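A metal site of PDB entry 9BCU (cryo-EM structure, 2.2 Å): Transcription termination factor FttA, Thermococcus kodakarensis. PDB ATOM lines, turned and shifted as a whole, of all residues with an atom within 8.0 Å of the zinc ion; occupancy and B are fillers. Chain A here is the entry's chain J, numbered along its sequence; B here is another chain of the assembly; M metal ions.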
ATOM      1  N   VAL A 197     -13.977  13.950   4.810  1.00  0.00           N
ATOM      2  CA  VAL A 197     -15.201  14.675   5.153  1.00  0.00           C
ATOM      3  C   VAL A 197     -14.814  15.947   5.892  1.00  0.00           C
ATOM      4  O   VAL A 197     -14.046  15.899   6.855  1.00  0.00           O
ATOM      5  CB  VAL A 197     -16.143  13.808   6.018  1.00  0.00           C
ATOM      6  CG1 VAL A 197     -17.506  14.462   6.125  1.00  0.00           C
ATOM      7  CG2 VAL A 197     -16.265  12.413   5.430  1.00  0.00           C
ATOM      8  N   GLY A 198     -15.330  17.073   5.423  1.00  0.00           N
ATOM      9  CA  GLY A 198     -15.056  18.363   6.021  1.00  0.00           C
ATOM     10  C   GLY A 198     -13.937  19.099   5.313  1.00  0.00           C
ATOM     11  O   GLY A 198     -13.265  18.581   4.412  1.00  0.00           O
ATOM     12  N   ARG A 199     -13.738  20.346   5.769  1.00  0.00           N
ATOM     13  CA  ARG A 199     -12.751  21.299   5.236  1.00  0.00           C
ATOM     14  C   ARG A 199     -12.658  21.258   3.711  1.00  0.00           C
ATOM     15  O   ARG A 199     -11.571  21.202   3.123  1.00  0.00           O
ATOM     16  CB  ARG A 199     -11.379  21.121   5.902  1.00  0.00           C
ATOM     17  CG  ARG A 199     -10.688  19.774   5.731  1.00  0.00           C
ATOM     18  CD  ARG A 199      -9.237  19.945   5.306  1.00  0.00           C
ATOM     19  NE  ARG A 199      -8.476  18.716   5.429  1.00  0.00           N
ATOM     20  CZ  ARG A 199      -7.154  18.640   5.283  1.00  0.00           C
ATOM     21  NH1 ARG A 199      -6.422  19.703   4.999  1.00  0.00           N
ATOM     22  NH2 ARG A 199      -6.560  17.446   5.415  1.00  0.00           N
ATOM     23  N   SER A 200     -13.817  21.289   3.073  1.00  0.00           N
ATOM     24  CA  SER A 200     -13.880  21.270   1.617  1.00  0.00           C
ATOM     25  C   SER A 200     -13.254  22.525   1.027  1.00  0.00           C
ATOM     26  O   SER A 200     -13.318  23.610   1.608  1.00  0.00           O
ATOM     27  CB  SER A 200     -15.324  21.134   1.141  1.00  0.00           C
ATOM     28  OG  SER A 200     -16.002  20.095   1.833  1.00  0.00           O
ATOM     29  N   ASP A 214     -16.701  26.522  -2.373  1.00  0.00           N
ATOM     30  CA  ASP A 214     -17.010  26.062  -0.998  1.00  0.00           C
ATOM     31  C   ASP A 214     -15.763  25.939  -0.114  1.00  0.00           C
ATOM     32  O   ASP A 214     -15.393  24.851   0.326  1.00  0.00           O
ATOM     33  CB  ASP A 214     -17.821  24.759  -0.983  1.00  0.00           C
ATOM     34  CG  ASP A 214     -17.288  23.676  -1.902  1.00  0.00           C
ATOM     35  OD1 ASP A 214     -16.205  23.120  -1.629  1.00  0.00           O
ATOM     36  OD2 ASP A 214     -17.992  23.326  -2.862  1.00  0.00           O
ATOM     37  N   THR A 252     -21.440  26.403  -1.906  1.00  0.00           N
ATOM     38  CA  THR A 252     -22.516  25.519  -2.324  1.00  0.00           C
ATOM     39  C   THR A 252     -23.722  25.626  -1.398  1.00  0.00           C
ATOM     40  O   THR A 252     -24.857  25.820  -1.841  1.00  0.00           O
ATOM     41  CB  THR A 252     -22.022  24.073  -2.383  1.00  0.00           C
ATOM     42  OG1 THR A 252     -21.252  23.781  -1.214  1.00  0.00           O
ATOM     43  CG2 THR A 252     -21.167  23.853  -3.620  1.00  0.00           C
ATOM     44  N   HIS A 253     -23.487  25.523  -0.094  1.00  0.00           N
ATOM     45  CA  HIS A 253     -24.564  25.624   0.883  1.00  0.00           C
ATOM     46  C   HIS A 253     -23.969  26.039   2.227  1.00  0.00           C
ATOM     47  O   HIS A 253     -22.755  25.966   2.440  1.00  0.00           O
ATOM     48  CB  HIS A 253     -25.343  24.312   1.004  1.00  0.00           C
ATOM     49  CG  HIS A 253     -24.600  23.228   1.723  1.00  0.00           C
ATOM     50  ND1 HIS A 253     -23.653  22.440   1.104  1.00  0.00           N
ATOM     51  CD2 HIS A 253     -24.688  22.784   3.001  1.00  0.00           C
ATOM     52  CE1 HIS A 253     -23.175  21.567   1.973  1.00  0.00           C
ATOM     53  NE2 HIS A 253     -23.783  21.750   3.130  1.00  0.00           N
ATOM     54  N   ALA A 255     -22.957  25.512   5.457  1.00  0.00           N
ATOM     55  CA  ALA A 255     -22.483  24.552   6.450  1.00  0.00           C
ATOM     56  C   ALA A 255     -21.037  24.866   6.785  1.00  0.00           C
ATOM     57  O   ALA A 255     -20.325  25.480   5.984  1.00  0.00           O
ATOM     58  CB  ALA A 255     -22.624  23.116   5.952  1.00  0.00           C
ATOM     59  N   LEU A 256     -20.595  24.446   7.979  1.00  0.00           N
ATOM     60  CA  LEU A 256     -19.257  24.789   8.433  1.00  0.00           C
ATOM     61  C   LEU A 256     -18.176  24.070   7.636  1.00  0.00           C
ATOM     62  O   LEU A 256     -17.044  24.559   7.555  1.00  0.00           O
ATOM     63  CB  LEU A 256     -19.116  24.475   9.922  1.00  0.00           C
ATOM     64  CG  LEU A 256     -19.871  25.418  10.858  1.00  0.00           C
ATOM     65  CD1 LEU A 256     -19.484  25.173  12.307  1.00  0.00           C
ATOM     66  CD2 LEU A 256     -19.629  26.874  10.474  1.00  0.00           C
ATOM     67  N   ASP A 257     -18.498  22.925   7.026  1.00  0.00           N
ATOM     68  CA  ASP A 257     -17.537  22.249   6.176  1.00  0.00           C
ATOM     69  C   ASP A 257     -17.493  22.832   4.764  1.00  0.00           C
ATOM     70  O   ASP A 257     -16.664  22.401   3.962  1.00  0.00           O
ATOM     71  CB  ASP A 257     -17.833  20.745   6.103  1.00  0.00           C
ATOM     72  CG  ASP A 257     -19.267  20.445   5.731  1.00  0.00           C
ATOM     73  OD1 ASP A 257     -20.172  21.098   6.281  1.00  0.00           O
ATOM     74  OD2 ASP A 257     -19.485  19.541   4.897  1.00  0.00           O
ATOM     75  N   HIS A 258     -18.364  23.788   4.450  1.00  0.00           N
ATOM     76  CA  HIS A 258     -18.345  24.470   3.163  1.00  0.00           C
ATOM     77  C   HIS A 258     -18.171  25.981   3.259  1.00  0.00           C
ATOM     78  O   HIS A 258     -17.835  26.603   2.252  1.00  0.00           O
ATOM     79  CB  HIS A 258     -19.629  24.168   2.374  1.00  0.00           C
ATOM     80  CG  HIS A 258     -19.759  22.746   1.952  1.00  0.00           C
ATOM     81  ND1 HIS A 258     -19.691  22.346   0.633  1.00  0.00           N
ATOM     82  CD2 HIS A 258     -19.964  21.618   2.675  1.00  0.00           C
ATOM     83  CE1 HIS A 258     -19.836  21.041   0.563  1.00  0.00           C
ATOM     84  NE2 HIS A 258     -20.004  20.562   1.791  1.00  0.00           N
ATOM     85  N   HIS A 341     -30.637  19.809  -0.224  1.00  0.00           N
ATOM     86  CA  HIS A 341     -30.052  19.400   1.050  1.00  0.00           C
ATOM     87  C   HIS A 341     -30.606  20.228   2.192  1.00  0.00           C
ATOM     88  O   HIS A 341     -31.251  19.698   3.107  1.00  0.00           O
ATOM     89  CB  HIS A 341     -28.531  19.511   0.977  1.00  0.00           C
ATOM     90  CG  HIS A 341     -27.839  19.046   2.227  1.00  0.00           C
ATOM     91  ND1 HIS A 341     -27.941  17.756   2.700  1.00  0.00           N
ATOM     92  CD2 HIS A 341     -27.048  19.705   3.106  1.00  0.00           C
ATOM     93  CE1 HIS A 341     -27.235  17.636   3.810  1.00  0.00           C
ATOM     94  NE2 HIS A 341     -26.680  18.807   4.076  1.00  0.00           N
ATOM     95  N   GLY A 363     -22.059  18.981  -4.507  1.00  0.00           N
ATOM     96  CA  GLY A 363     -21.953  19.120  -3.065  1.00  0.00           C
ATOM     97  C   GLY A 363     -22.971  18.238  -2.355  1.00  0.00           C
ATOM     98  O   GLY A 363     -23.364  17.173  -2.852  1.00  0.00           O
ATOM     99  N   ASP A 364     -23.388  18.681  -1.181  1.00  0.00           N
ATOM    100  CA  ASP A 364     -24.449  17.984  -0.462  1.00  0.00           C
ATOM    101  C   ASP A 364     -25.785  18.213  -1.165  1.00  0.00           C
ATOM    102  O   ASP A 364     -26.161  19.357  -1.433  1.00  0.00           O
ATOM    103  CB  ASP A 364     -24.517  18.457   0.986  1.00  0.00           C
ATOM    104  CG  ASP A 364     -23.553  17.710   1.886  1.00  0.00           C
ATOM    105  OD1 ASP A 364     -23.662  16.478   1.987  1.00  0.00           O
ATOM    106  OD2 ASP A 364     -22.679  18.366   2.497  1.00  0.00           O
ATOM    107  N   PHE A 365     -26.501  17.122  -1.448  1.00  0.00           N
ATOM    108  CA  PHE A 365     -27.752  17.221  -2.182  1.00  0.00           C
ATOM    109  C   PHE A 365     -28.611  16.005  -1.881  1.00  0.00           C
ATOM    110  O   PHE A 365     -28.136  15.004  -1.333  1.00  0.00           O
ATOM    111  CB  PHE A 365     -27.504  17.346  -3.699  1.00  0.00           C
ATOM    112  CG  PHE A 365     -27.104  16.049  -4.346  1.00  0.00           C
ATOM    113  CD1 PHE A 365     -25.828  15.542  -4.197  1.00  0.00           C
ATOM    114  CD2 PHE A 365     -28.009  15.344  -5.134  1.00  0.00           C
ATOM    115  CE1 PHE A 365     -25.460  14.354  -4.802  1.00  0.00           C
ATOM    116  CE2 PHE A 365     -27.647  14.149  -5.736  1.00  0.00           C
ATOM    117  CZ  PHE A 365     -26.363  13.659  -5.570  1.00  0.00           C
ATOM    118  N   GLU A 389     -20.813  14.369  -4.260  1.00  0.00           N
ATOM    119  CA  GLU A 389     -20.511  13.977  -2.899  1.00  0.00           C
ATOM    120  C   GLU A 389     -20.563  12.458  -2.760  1.00  0.00           C
ATOM    121  O   GLU A 389     -21.235  11.761  -3.519  1.00  0.00           O
ATOM    122  CB  GLU A 389     -21.467  14.639  -1.919  1.00  0.00           C
ATOM    123  CG  GLU A 389     -22.873  14.068  -1.938  1.00  0.00           C
ATOM    124  CD  GLU A 389     -23.537  14.106  -0.575  1.00  0.00           C
ATOM    125  OE1 GLU A 389     -22.821  14.149   0.440  1.00  0.00           O
ATOM    126  OE2 GLU A 389     -24.787  14.112  -0.522  1.00  0.00           O
ATOM    127  N   THR A 391     -20.789  10.975   0.691  1.00  0.00           N
ATOM    128  CA  THR A 391     -20.993  10.765   2.119  1.00  0.00           C
ATOM    129  C   THR A 391     -21.559   9.379   2.397  1.00  0.00           C
ATOM    130  O   THR A 391     -21.139   8.700   3.346  1.00  0.00           O
ATOM    131  CB  THR A 391     -21.901  11.846   2.700  1.00  0.00           C
ATOM    132  OG1 THR A 391     -21.456  13.134   2.261  1.00  0.00           O
ATOM    133  CG2 THR A 391     -21.885  11.804   4.213  1.00  0.00           C
ATOM    134  N   HIS A 615     -15.961  14.467  -1.021  1.00  0.00           N
ATOM    135  CA  HIS A 615     -16.798  14.698   0.155  1.00  0.00           C
ATOM    136  C   HIS A 615     -17.281  13.374   0.772  1.00  0.00           C
ATOM    137  O   HIS A 615     -18.477  13.083   0.843  1.00  0.00           O
ATOM    138  CB  HIS A 615     -17.973  15.615  -0.182  1.00  0.00           C
ATOM    139  CG  HIS A 615     -18.645  16.211   1.029  1.00  0.00           C
ATOM    140  ND1 HIS A 615     -19.806  15.702   1.562  1.00  0.00           N
ATOM    141  CD2 HIS A 615     -18.306  17.266   1.803  1.00  0.00           C
ATOM    142  CE1 HIS A 615     -20.157  16.421   2.608  1.00  0.00           C
ATOM    143  NE2 HIS A 615     -19.261  17.375   2.784  1.00  0.00           N
ATOM    144  P     U B  15     -21.731  15.817  13.068  1.00  0.00           P
ATOM    145  OP1   U B  15     -23.049  15.185  13.381  1.00  0.00           O
ATOM    146  OP2   U B  15     -21.054  15.470  11.792  1.00  0.00           O
ATOM    147  O5'   U B  15     -21.929  17.390  13.120  1.00  0.00           O
ATOM    148  C5'   U B  15     -22.375  18.117  11.974  1.00  0.00           C
ATOM    149  C4'   U B  15     -21.595  19.397  11.799  1.00  0.00           C
ATOM    150  O4'   U B  15     -20.176  19.108  11.874  1.00  0.00           O
ATOM    151  C3'   U B  15     -21.820  20.109  10.471  1.00  0.00           C
ATOM    152  O3'   U B  15     -21.723  21.521  10.663  1.00  0.00           O
ATOM    153  C2'   U B  15     -20.653  19.622   9.624  1.00  0.00           C
ATOM    154  O2'   U B  15     -20.294  20.486   8.577  1.00  0.00           O
ATOM    155  C1'   U B  15     -19.544  19.520  10.669  1.00  0.00           C
ATOM    156  N1    U B  15     -18.503  18.530  10.346  1.00  0.00           N
ATOM    157  C2    U B  15     -17.281  18.990   9.908  1.00  0.00           C
ATOM    158  O2    U B  15     -17.023  20.182   9.782  1.00  0.00           O
ATOM    159  N3    U B  15     -16.361  18.017   9.628  1.00  0.00           N
ATOM    160  C4    U B  15     -16.538  16.654   9.731  1.00  0.00           C
ATOM    161  O4    U B  15     -15.610  15.901   9.428  1.00  0.00           O
ATOM    162  C5    U B  15     -17.831  16.253  10.187  1.00  0.00           C
ATOM    163  C6    U B  15     -18.745  17.186  10.466  1.00  0.00           C
ATOM    164  P     U B  16     -23.029  22.446  10.617  1.00  0.00           P
ATOM    165  OP1   U B  16     -24.133  21.653  10.016  1.00  0.00           O
ATOM    166  OP2   U B  16     -22.658  23.748  10.025  1.00  0.00           O
ATOM    167  O5'   U B  16     -23.386  22.682  12.151  1.00  0.00           O
ATOM    168  C5'   U B  16     -22.344  22.796  13.123  1.00  0.00           C
ATOM    169  C4'   U B  16     -22.721  22.146  14.429  1.00  0.00           C
ATOM    170  O4'   U B  16     -21.500  21.793  15.139  1.00  0.00           O
ATOM    171  C3'   U B  16     -23.529  23.016  15.388  1.00  0.00           C
ATOM    172  O3'   U B  16     -24.428  22.203  16.145  1.00  0.00           O
ATOM    173  C2'   U B  16     -22.462  23.579  16.310  1.00  0.00           C
ATOM    174  O2'   U B  16     -22.928  23.973  17.585  1.00  0.00           O
ATOM    175  C1'   U B  16     -21.487  22.401  16.415  1.00  0.00           C
ATOM    176  N1    U B  16     -20.106  22.802  16.715  1.00  0.00           N
ATOM    177  C2    U B  16     -19.463  22.164  17.759  1.00  0.00           C
ATOM    178  O2    U B  16     -19.982  21.278  18.415  1.00  0.00           O
ATOM    179  N3    U B  16     -18.180  22.589  17.988  1.00  0.00           N
ATOM    180  C4    U B  16     -17.496  23.578  17.304  1.00  0.00           C
ATOM    181  O4    U B  16     -16.342  23.851  17.635  1.00  0.00           O
ATOM    182  C5    U B  16     -18.237  24.198  16.258  1.00  0.00           C
ATOM    183  C6    U B  16     -19.489  23.801  15.998  1.00  0.00           C
HETATM  184 ZN    ZN M   1     -20.790  19.014   3.289  1.00  0.00          ZN
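The zinc ion is bound by the side-chain carboxylate of Asp 257 (2.1 Å), the side-chain carboxylate of Asp 364 (2.1 Å), a ring nitrogen (NE2) of His 258 (2.3 Å) and a ring nitrogen (NE2) of His 615 (2.3 Å). The zinc ion has four donor atoms within binding distance.
Residues that only touch the zinc ion: His 253 (3.7 Å). Of the 20 residues printed, 5 come within 4 Å of the zinc ion.
N of Ser 200 is in hydrogen-bond range of O of Asp 257, 3.2 Å away. N of Asp 257 lies close to O2' of U 15 of chain B (3.4 Å). The side-chain hydroxyl of Thr 252 lies within hydrogen-bond range of a ring nitrogen (ND1) of His 258 (2.8 Å). ND1 of His 615 sits at hydrogen-bond distance from OG1 of Thr 391 (3.1 Å).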
